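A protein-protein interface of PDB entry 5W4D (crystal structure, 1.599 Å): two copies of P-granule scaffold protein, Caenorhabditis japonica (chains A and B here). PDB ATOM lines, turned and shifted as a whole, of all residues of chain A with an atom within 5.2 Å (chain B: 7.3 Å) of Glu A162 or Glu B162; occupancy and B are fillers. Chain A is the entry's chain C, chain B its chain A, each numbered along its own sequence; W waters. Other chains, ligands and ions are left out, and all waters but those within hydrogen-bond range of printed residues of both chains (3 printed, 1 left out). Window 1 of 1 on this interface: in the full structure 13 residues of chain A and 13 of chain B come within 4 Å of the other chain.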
ATOM      1  N   LYS A 131     -27.765  -0.164  -1.670  1.00  0.00           N
ATOM      2  CA  LYS A 131     -28.073   0.751  -0.568  1.00  0.00           C
ATOM      3  C   LYS A 131     -29.572   0.867  -0.345  1.00  0.00           C
ATOM      4  O   LYS A 131     -30.022   1.120   0.782  1.00  0.00           O
ATOM      5  CB  LYS A 131     -27.458   2.119  -0.826  1.00  0.00           C
ATOM      6  CG  LYS A 131     -27.458   3.012   0.403  1.00  0.00           C
ATOM      7  CD  LYS A 131     -26.575   4.204   0.213  1.00  0.00           C
ATOM      8  CE  LYS A 131     -26.417   4.957   1.540  1.00  0.00           C
ATOM      9  NZ  LYS A 131     -25.639   6.164   1.353  1.00  0.00           N
ATOM     10  N   ILE A 143     -21.612   0.599   0.975  1.00  0.00           N
ATOM     11  CA  ILE A 143     -20.562   1.481   1.498  1.00  0.00           C
ATOM     12  C   ILE A 143     -19.172   1.022   1.060  1.00  0.00           C
ATOM     13  O   ILE A 143     -18.319   1.838   0.671  1.00  0.00           O
ATOM     14  CB  ILE A 143     -20.679   1.577   3.029  1.00  0.00           C
ATOM     15  CG1 ILE A 143     -21.977   2.256   3.374  1.00  0.00           C
ATOM     16  CG2 ILE A 143     -19.461   2.338   3.600  1.00  0.00           C
ATOM     17  CD1 ILE A 143     -22.355   2.100   4.876  1.00  0.00           C
ATOM     18  N   THR A 158     -15.816  10.766   3.045  1.00  0.00           N
ATOM     19  CA  THR A 158     -17.252  11.013   2.950  1.00  0.00           C
ATOM     20  C   THR A 158     -18.029   9.710   2.804  1.00  0.00           C
ATOM     21  O   THR A 158     -19.067   9.513   3.452  1.00  0.00           O
ATOM     22  CB  THR A 158     -17.546  11.950   1.775  1.00  0.00           C
ATOM     23  OG1 THR A 158     -16.879  13.191   1.999  1.00  0.00           O
ATOM     24  CG2 THR A 158     -19.018  12.247   1.613  1.00  0.00           C
ATOM     25  N   GLU A 159     -17.522   8.786   1.999  1.00  0.00           N
ATOM     26  CA  GLU A 159     -18.259   7.529   1.827  1.00  0.00           C
ATOM     27  C   GLU A 159     -18.144   6.640   3.065  1.00  0.00           C
ATOM     28  O   GLU A 159     -19.142   6.044   3.498  1.00  0.00           O
ATOM     29  CB  GLU A 159     -17.784   6.806   0.584  1.00  0.00           C
ATOM     30  CG  GLU A 159     -18.054   7.607  -0.707  1.00  0.00           C
ATOM     31  CD  GLU A 159     -19.569   7.825  -1.034  1.00  0.00           C
ATOM     32  OE1 GLU A 159     -20.477   7.304  -0.337  1.00  0.00           O
ATOM     33  OE2 GLU A 159     -19.856   8.525  -2.049  1.00  0.00           O
ATOM     34  N   LEU A 160     -16.946   6.567   3.677  1.00  0.00           N
ATOM     35  CA  LEU A 160     -16.768   5.778   4.909  1.00  0.00           C
ATOM     36  C   LEU A 160     -17.614   6.313   6.063  1.00  0.00           C
ATOM     37  O   LEU A 160     -18.019   5.551   6.960  1.00  0.00           O
ATOM     38  CB  LEU A 160     -15.288   5.763   5.302  1.00  0.00           C
ATOM     39  CG  LEU A 160     -14.438   4.846   4.422  1.00  0.00           C
ATOM     40  CD1 LEU A 160     -13.002   5.172   4.625  1.00  0.00           C
ATOM     41  CD2 LEU A 160     -14.721   3.368   4.749  1.00  0.00           C
ATOM     42  N   SER A 161     -17.868   7.633   6.073  1.00  0.00           N
ATOM     43  CA  SER A 161     -18.679   8.244   7.121  1.00  0.00           C
ATOM     44  C   SER A 161     -20.071   7.637   7.192  1.00  0.00           C
ATOM     45  O   SER A 161     -20.684   7.617   8.260  1.00  0.00           O
ATOM     46  CB  SER A 161     -18.777   9.761   6.898  1.00  0.00           C
ATOM     47  OG  SER A 161     -17.550  10.398   7.198  1.00  0.00           O
ATOM     48  N   GLU A 162     -20.568   7.113   6.064  1.00  0.00           N
ATOM     49  CA  GLU A 162     -21.872   6.454   6.044  1.00  0.00           C
ATOM     50  C   GLU A 162     -21.936   5.262   6.986  1.00  0.00           C
ATOM     51  O   GLU A 162     -23.052   4.838   7.365  1.00  0.00           O
ATOM     52  CB  GLU A 162     -22.234   6.018   4.619  1.00  0.00           C
ATOM     53  CG  GLU A 162     -22.442   7.199   3.641  1.00  0.00           C
ATOM     54  CD  GLU A 162     -23.687   7.983   3.989  1.00  0.00           C
ATOM     55  OE1 GLU A 162     -24.726   7.338   4.229  1.00  0.00           O
ATOM     56  OE2 GLU A 162     -23.604   9.234   4.106  1.00  0.00           O
ATOM     57  N   LEU A 163     -20.779   4.699   7.366  1.00  0.00           N
ATOM     58  CA  LEU A 163     -20.781   3.628   8.360  1.00  0.00           C
ATOM     59  C   LEU A 163     -21.448   4.075   9.659  1.00  0.00           C
ATOM     60  O   LEU A 163     -22.029   3.257  10.374  1.00  0.00           O
ATOM     61  CB  LEU A 163     -19.348   3.158   8.646  1.00  0.00           C
ATOM     62  CG  LEU A 163     -18.718   2.399   7.480  1.00  0.00           C
ATOM     63  CD1 LEU A 163     -17.208   2.218   7.699  1.00  0.00           C
ATOM     64  CD2 LEU A 163     -19.355   1.021   7.253  1.00  0.00           C
ATOM     65  N   CYS A 164     -21.368   5.364   9.998  1.00  0.00           N
ATOM     66  CA  CYS A 164     -21.996   5.850  11.216  1.00  0.00           C
ATOM     67  C   CYS A 164     -23.517   5.674  11.188  1.00  0.00           C
ATOM     68  O   CYS A 164     -24.136   5.538  12.243  1.00  0.00           O
ATOM     69  CB  CYS A 164     -21.625   7.305  11.413  1.00  0.00           C
ATOM     70  SG  CYS A 164     -19.799   7.516  11.600  1.00  0.00           S
ATOM     71  N   GLY A 165     -24.118   5.635  10.000  1.00  0.00           N
ATOM     72  CA  GLY A 165     -25.546   5.397   9.860  1.00  0.00           C
ATOM     73  C   GLY A 165     -25.986   3.990  10.225  1.00  0.00           C
ATOM     74  O   GLY A 165     -27.187   3.751  10.419  1.00  0.00           O
ATOM     75  N   LEU A 166     -25.043   3.051  10.292  1.00  0.00           N
ATOM     76  CA  LEU A 166     -25.246   1.698  10.809  1.00  0.00           C
ATOM     77  C   LEU A 166     -24.713   1.523  12.231  1.00  0.00           C
ATOM     78  O   LEU A 166     -24.608   0.383  12.710  1.00  0.00           O
ATOM     79  CB  LEU A 166     -24.573   0.662   9.897  1.00  0.00           C
ATOM     80  CG  LEU A 166     -25.018   0.709   8.444  1.00  0.00           C
ATOM     81  CD1 LEU A 166     -24.194  -0.192   7.536  1.00  0.00           C
ATOM     82  CD2 LEU A 166     -26.484   0.275   8.385  1.00  0.00           C
ATOM     83  N   LYS B 131     -25.750  14.742   9.693  1.00  0.00           N
ATOM     84  CA  LYS B 131     -25.926  13.355   9.290  1.00  0.00           C
ATOM     85  C   LYS B 131     -25.275  12.390  10.280  1.00  0.00           C
ATOM     86  O   LYS B 131     -25.771  11.273  10.462  1.00  0.00           O
ATOM     87  CB  LYS B 131     -25.363  13.129   7.883  1.00  0.00           C
ATOM     88  CG  LYS B 131     -25.790  11.804   7.288  1.00  0.00           C
ATOM     89  CD  LYS B 131     -25.455  11.739   5.829  1.00  0.00           C
ATOM     90  CE  LYS B 131     -26.028  10.446   5.210  1.00  0.00           C
ATOM     91  NZ  LYS B 131     -25.782  10.412   3.735  1.00  0.00           N
ATOM     92  N   LEU B 132     -24.197  12.828  10.948  1.00  0.00           N
ATOM     93  CA  LEU B 132     -23.482  11.998  11.916  1.00  0.00           C
ATOM     94  C   LEU B 132     -24.167  11.933  13.275  1.00  0.00           C
ATOM     95  O   LEU B 132     -23.774  11.114  14.111  1.00  0.00           O
ATOM     96  CB  LEU B 132     -22.052  12.538  12.096  1.00  0.00           C
ATOM     97  CG  LEU B 132     -21.186  12.547  10.842  1.00  0.00           C
ATOM     98  CD1 LEU B 132     -19.864  13.308  11.117  1.00  0.00           C
ATOM     99  CD2 LEU B 132     -20.892  11.159  10.254  1.00  0.00           C
ATOM    100  N   LYS B 139     -30.977  13.573  10.734  1.00  0.00           N
ATOM    101  CA  LYS B 139     -30.758  12.916   9.442  1.00  0.00           C
ATOM    102  C   LYS B 139     -31.680  13.487   8.367  1.00  0.00           C
ATOM    103  O   LYS B 139     -31.254  13.676   7.222  1.00  0.00           O
ATOM    104  CB  LYS B 139     -30.923  11.406   9.585  1.00  0.00           C
ATOM    105  CG  LYS B 139     -29.806  10.775  10.430  1.00  0.00           C
ATOM    106  CD  LYS B 139     -30.123   9.383  10.835  1.00  0.00           C
ATOM    107  CE  LYS B 139     -29.101   8.878  11.857  1.00  0.00           C
ATOM    108  NZ  LYS B 139     -27.686   9.065  11.409  1.00  0.00           N
ATOM    109  N   ILE B 143     -30.355  15.342   4.849  1.00  0.00           N
ATOM    110  CA  ILE B 143     -30.820  15.002   3.503  1.00  0.00           C
ATOM    111  C   ILE B 143     -31.401  16.224   2.809  1.00  0.00           C
ATOM    112  O   ILE B 143     -31.176  16.448   1.613  1.00  0.00           O
ATOM    113  CB  ILE B 143     -31.838  13.846   3.573  1.00  0.00           C
ATOM    114  CG1 ILE B 143     -31.089  12.587   3.999  1.00  0.00           C
ATOM    115  CG2 ILE B 143     -32.543  13.652   2.220  1.00  0.00           C
ATOM    116  CD1 ILE B 143     -32.019  11.473   4.522  1.00  0.00           C
ATOM    117  N   LYS B 146     -28.525  18.448   1.663  1.00  0.00           N
ATOM    118  CA  LYS B 146     -27.848  17.869   0.506  1.00  0.00           C
ATOM    119  C   LYS B 146     -28.684  17.989  -0.769  1.00  0.00           C
ATOM    120  O   LYS B 146     -28.129  18.189  -1.869  1.00  0.00           O
ATOM    121  CB  LYS B 146     -27.515  16.414   0.829  1.00  0.00           C
ATOM    122  CG  LYS B 146     -26.437  16.355   1.898  1.00  0.00           C
ATOM    123  CD  LYS B 146     -26.168  14.971   2.347  1.00  0.00           C
ATOM    124  CE  LYS B 146     -25.136  14.939   3.509  1.00  0.00           C
ATOM    125  NZ  LYS B 146     -23.852  15.486   3.055  1.00  0.00           N
ATOM    126  N   LYS B 156     -29.541  15.373  -7.384  1.00  0.00           N
ATOM    127  CA  LYS B 156     -30.708  15.542  -6.522  1.00  0.00           C
ATOM    128  C   LYS B 156     -31.383  14.204  -6.241  1.00  0.00           C
ATOM    129  O   LYS B 156     -31.729  13.886  -5.084  1.00  0.00           O
ATOM    130  CB  LYS B 156     -31.671  16.555  -7.155  1.00  0.00           C
ATOM    131  CG  LYS B 156     -32.597  17.129  -6.199  1.00  0.00           C
ATOM    132  CD  LYS B 156     -33.434  18.235  -6.816  1.00  0.00           C
ATOM    133  CE  LYS B 156     -34.286  18.864  -5.710  1.00  0.00           C
ATOM    134  NZ  LYS B 156     -34.912  20.188  -6.072  1.00  0.00           N
ATOM    135  N   PHE B 157     -31.522  13.371  -7.270  1.00  0.00           N
ATOM    136  CA  PHE B 157     -32.088  12.045  -7.070  1.00  0.00           C
ATOM    137  C   PHE B 157     -31.236  11.196  -6.137  1.00  0.00           C
ATOM    138  O   PHE B 157     -31.771  10.475  -5.279  1.00  0.00           O
ATOM    139  CB  PHE B 157     -32.232  11.338  -8.418  1.00  0.00           C
ATOM    140  CG  PHE B 157     -32.754   9.945  -8.281  1.00  0.00           C
ATOM    141  CD1 PHE B 157     -34.074   9.718  -7.917  1.00  0.00           C
ATOM    142  CD2 PHE B 157     -31.923   8.863  -8.464  1.00  0.00           C
ATOM    143  CE1 PHE B 157     -34.575   8.432  -7.776  1.00  0.00           C
ATOM    144  CE2 PHE B 157     -32.407   7.573  -8.313  1.00  0.00           C
ATOM    145  CZ  PHE B 157     -33.737   7.357  -7.963  1.00  0.00           C
ATOM    146  N   THR B 158     -29.905  11.235  -6.314  1.00  0.00           N
ATOM    147  CA  THR B 158     -29.015  10.470  -5.436  1.00  0.00           C
ATOM    148  C   THR B 158     -29.160  10.887  -3.974  1.00  0.00           C
ATOM    149  O   THR B 158     -29.221  10.029  -3.070  1.00  0.00           O
ATOM    150  CB  THR B 158     -27.570  10.666  -5.896  1.00  0.00           C
ATOM    151  OG1 THR B 158     -27.427  10.186  -7.253  1.00  0.00           O
ATOM    152  CG2 THR B 158     -26.583   9.939  -4.998  1.00  0.00           C
ATOM    153  N   GLU B 159     -29.241  12.192  -3.715  1.00  0.00           N
ATOM    154  CA  GLU B 159     -29.397  12.658  -2.322  1.00  0.00           C
ATOM    155  C   GLU B 159     -30.795  12.344  -1.765  1.00  0.00           C
ATOM    156  O   GLU B 159     -30.927  11.886  -0.623  1.00  0.00           O
ATOM    157  CB  GLU B 159     -29.071  14.157  -2.234  1.00  0.00           C
ATOM    158  CG  GLU B 159     -27.598  14.496  -2.609  1.00  0.00           C
ATOM    159  CD  GLU B 159     -26.515  13.847  -1.721  1.00  0.00           C
ATOM    160  OE1 GLU B 159     -26.787  13.215  -0.678  1.00  0.00           O
ATOM    161  OE2 GLU B 159     -25.315  13.973  -2.086  1.00  0.00           O
ATOM    162  N   LEU B 160     -31.861  12.530  -2.560  1.00  0.00           N
ATOM    163  CA  LEU B 160     -33.193  12.182  -2.070  1.00  0.00           C
ATOM    164  C   LEU B 160     -33.343  10.683  -1.826  1.00  0.00           C
ATOM    165  O   LEU B 160     -34.142  10.264  -0.971  1.00  0.00           O
ATOM    166  CB  LEU B 160     -34.249  12.644  -3.065  1.00  0.00           C
ATOM    167  CG  LEU B 160     -34.494  14.144  -3.096  1.00  0.00           C
ATOM    168  CD1 LEU B 160     -35.231  14.500  -4.373  1.00  0.00           C
ATOM    169  CD2 LEU B 160     -35.263  14.571  -1.858  1.00  0.00           C
ATOM    170  N   SER B 161     -32.594   9.857  -2.565  1.00  0.00           N
ATOM    171  CA  SER B 161     -32.630   8.417  -2.334  1.00  0.00           C
ATOM    172  C   SER B 161     -32.262   8.049  -0.899  1.00  0.00           C
ATOM    173  O   SER B 161     -32.676   6.987  -0.415  1.00  0.00           O
ATOM    174  CB  SER B 161     -31.700   7.710  -3.328  1.00  0.00           C
ATOM    175  OG  SER B 161     -32.281   7.712  -4.647  1.00  0.00           O
ATOM    176  N   GLU B 162     -31.451   8.877  -0.228  1.00  0.00           N
ATOM    177  CA  GLU B 162     -31.101   8.599   1.167  1.00  0.00           C
ATOM    178  C   GLU B 162     -32.320   8.554   2.086  1.00  0.00           C
ATOM    179  O   GLU B 162     -32.235   7.992   3.193  1.00  0.00           O
ATOM    180  CB  GLU B 162     -30.099   9.629   1.656  1.00  0.00           C
ATOM    181  CG  GLU B 162     -28.771   9.557   0.887  1.00  0.00           C
ATOM    182  CD  GLU B 162     -27.983   8.327   1.236  1.00  0.00           C
ATOM    183  OE1 GLU B 162     -27.889   8.036   2.445  1.00  0.00           O
ATOM    184  OE2 GLU B 162     -27.513   7.614   0.310  1.00  0.00           O
ATOM    185  N   LEU B 163     -33.445   9.157   1.678  1.00  0.00           N
ATOM    186  CA  LEU B 163     -34.672   9.047   2.463  1.00  0.00           C
ATOM    187  C   LEU B 163     -35.059   7.598   2.697  1.00  0.00           C
ATOM    188  O   LEU B 163     -35.718   7.265   3.707  1.00  0.00           O
ATOM    189  CB  LEU B 163     -35.819   9.788   1.775  1.00  0.00           C
ATOM    190  CG  LEU B 163     -35.654  11.323   1.749  1.00  0.00           C
ATOM    191  CD1 LEU B 163     -36.694  11.999   0.831  1.00  0.00           C
ATOM    192  CD2 LEU B 163     -35.677  11.925   3.183  1.00  0.00           C
ATOM    193  N   CYS B 164     -34.710   6.706   1.759  1.00  0.00           N
ATOM    194  CA  CYS B 164     -35.049   5.297   1.922  1.00  0.00           C
ATOM    195  C   CYS B 164     -34.348   4.692   3.141  1.00  0.00           C
ATOM    196  O   CYS B 164     -34.858   3.740   3.738  1.00  0.00           O
ATOM    197  CB  CYS B 164     -34.704   4.520   0.650  1.00  0.00           C
ATOM    198  SG  CYS B 164     -35.628   5.180  -0.832  1.00  0.00           S
ATOM    199  N   GLY B 165     -33.217   5.254   3.551  1.00  0.00           N
ATOM    200  CA  GLY B 165     -32.539   4.759   4.744  1.00  0.00           C
ATOM    201  C   GLY B 165     -33.295   5.018   6.033  1.00  0.00           C
ATOM    202  O   GLY B 165     -32.967   4.416   7.066  1.00  0.00           O
ATOM    203  N   LEU B 166     -34.261   5.948   5.999  1.00  0.00           N
ATOM    204  CA  LEU B 166     -35.180   6.250   7.097  1.00  0.00           C
ATOM    205  C   LEU B 166     -36.551   5.627   6.855  1.00  0.00           C
ATOM    206  O   LEU B 166     -37.526   5.969   7.545  1.00  0.00           O
ATOM    207  CB  LEU B 166     -35.342   7.765   7.266  1.00  0.00           C
ATOM    208  CG  LEU B 166     -34.061   8.551   7.456  1.00  0.00           C
ATOM    209  CD1 LEU B 166     -34.291  10.054   7.423  1.00  0.00           C
ATOM    210  CD2 LEU B 166     -33.514   8.166   8.812  1.00  0.00           C
ATOM    211  N   ASP B 167     -36.653   4.728   5.871  1.00  0.00           N
ATOM    212  CA  ASP B 167     -37.918   4.140   5.456  1.00  0.00           C
ATOM    213  C   ASP B 167     -38.908   5.221   5.042  1.00  0.00           C
ATOM    214  O   ASP B 167     -40.114   5.104   5.246  1.00  0.00           O
ATOM    215  CB  ASP B 167     -38.488   3.217   6.536  1.00  0.00           C
ATOM    216  CG  ASP B 167     -37.680   1.923   6.699  1.00  0.00           C
ATOM    217  OD1 ASP B 167     -36.780   1.628   5.891  1.00  0.00           O
ATOM    218  OD2 ASP B 167     -37.959   1.188   7.669  1.00  0.00           O
ATOM    219  N   LEU B 168     -38.380   6.262   4.405  1.00  0.00           N
ATOM    220  CA  LEU B 168     -39.173   7.318   3.782  1.00  0.00           C
ATOM    221  C   LEU B 168     -39.224   7.148   2.256  1.00  0.00           C
ATOM    222  O   LEU B 168     -39.224   8.102   1.472  1.00  0.00           O
ATOM    223  CB  LEU B 168     -38.632   8.685   4.204  1.00  0.00           C
ATOM    224  CG  LEU B 168     -38.872   9.043   5.673  1.00  0.00           C
ATOM    225  CD1 LEU B 168     -38.202  10.326   5.942  1.00  0.00           C
ATOM    226  CD2 LEU B 168     -40.372   9.144   5.980  1.00  0.00           C
ATOM    227  N   ALA B 172     -39.402   9.789  -1.106  1.00  0.00           N
ATOM    228  CA  ALA B 172     -38.467   9.713  -2.227  1.00  0.00           C
ATOM    229  C   ALA B 172     -39.217   9.510  -3.533  1.00  0.00           C
ATOM    230  O   ALA B 172     -38.883  10.126  -4.548  1.00  0.00           O
ATOM    231  CB  ALA B 172     -37.456   8.602  -2.017  1.00  0.00           C
ATOM    232  N   ILE B 193     -37.253   1.799  -5.294  1.00  0.00           N
ATOM    233  CA  ILE B 193     -37.933   2.704  -4.357  1.00  0.00           C
ATOM    234  C   ILE B 193     -39.434   2.461  -4.369  1.00  0.00           C
ATOM    235  O   ILE B 193     -40.055   2.308  -3.313  1.00  0.00           O
ATOM    236  CB  ILE B 193     -37.586   4.171  -4.679  1.00  0.00           C
ATOM    237  CG1 ILE B 193     -36.084   4.419  -4.503  1.00  0.00           C
ATOM    238  CG2 ILE B 193     -38.400   5.099  -3.785  1.00  0.00           C
ATOM    239  CD1 ILE B 193     -35.637   5.805  -4.945  1.00  0.00           C
HETATM  240  O   HOH W   1     -31.789   2.774   1.851  1.00  0.00           O
HETATM  241  O   HOH W   2     -24.073   8.522  13.313  1.00  0.00           O
HETATM  242  O   HOH W   3     -24.759   8.745  10.648  1.00  0.00           O
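NZ of Lys A131 is in salt-bridge range of OE2 of Glu B162 (2.6 Å). The side-chain amino group (NZ) of Lys B131 lies within salt-bridge range of the side-chain carboxylate (OE2) of Glu A162 (2.5 Å).
NZ of Lys A131 lies within salt-bridge range of OE1 of Glu A162 (3.2 Å). The side-chain amino group (NZ) of Lys B139 is in hydrogen-bond range of the backbone carbonyl oxygen (O) of Lys B131 (3.1 Å). NZ of Lys B131 lies within salt-bridge range of OE1 of Glu B162, 3.4 Å away.
Glu A162 touches Glu B162 (OE1 to OE1, 3.7 Å).
Of the printed residues of chain B, Glu A162 touches Lys B131 (2.5 Å) and Glu B162 (3.7 Å). Of chain A, only Lys A131 (2.6 Å) and Glu A162 (3.7 Å) come within 4 Å of Glu B162. Of the printed residues of chain A, Lys B131 touches Glu A162 (2.5 Å). Printed residues of chain B within 4 Å of Lys A131: Glu B162. The nearest printed residue of chain A that does not touch Glu B162 is Glu A159 (7.1 Å). The nearest printed residue of chain B that does not touch Lys A131 is Lys B131 (4.9 Å).
Of the 20 printed residues of chain B, 2 touch a printed residue of chain A. Among the printed residues, Asp or Glu carboxylates within 4 Å of a Lys or Arg side-chain nitrogen of the other chain: Lys A131 with Glu B162 and Glu A162 with Lys B131.
Lys A131 touches Glu B162, and with the chains exchanged Glu A162 touches Lys B131. Glu B162 touches its own counterpart, Glu A162. Positions printed for both chains: 131, 143, 158, 159, 160, 161, 162, 163, 164, 165 and 166.
Water W1 bridges the backbone carbonyl oxygen of Lys A131 (2.6 Å) and the backbone NH of Gly B165 (3.3 Å). Water W2 bridges O of Leu B132 (2.7 Å) and O of Cys A164 (3.2 Å). Water W3 lies within hydrogen-bond range of the backbone carbonyl oxygen of Lys B131 (2.7 Å), the side-chain amino group of Lys B139 (3.0 Å) and the backbone NH of Gly A165 (3.2 Å).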
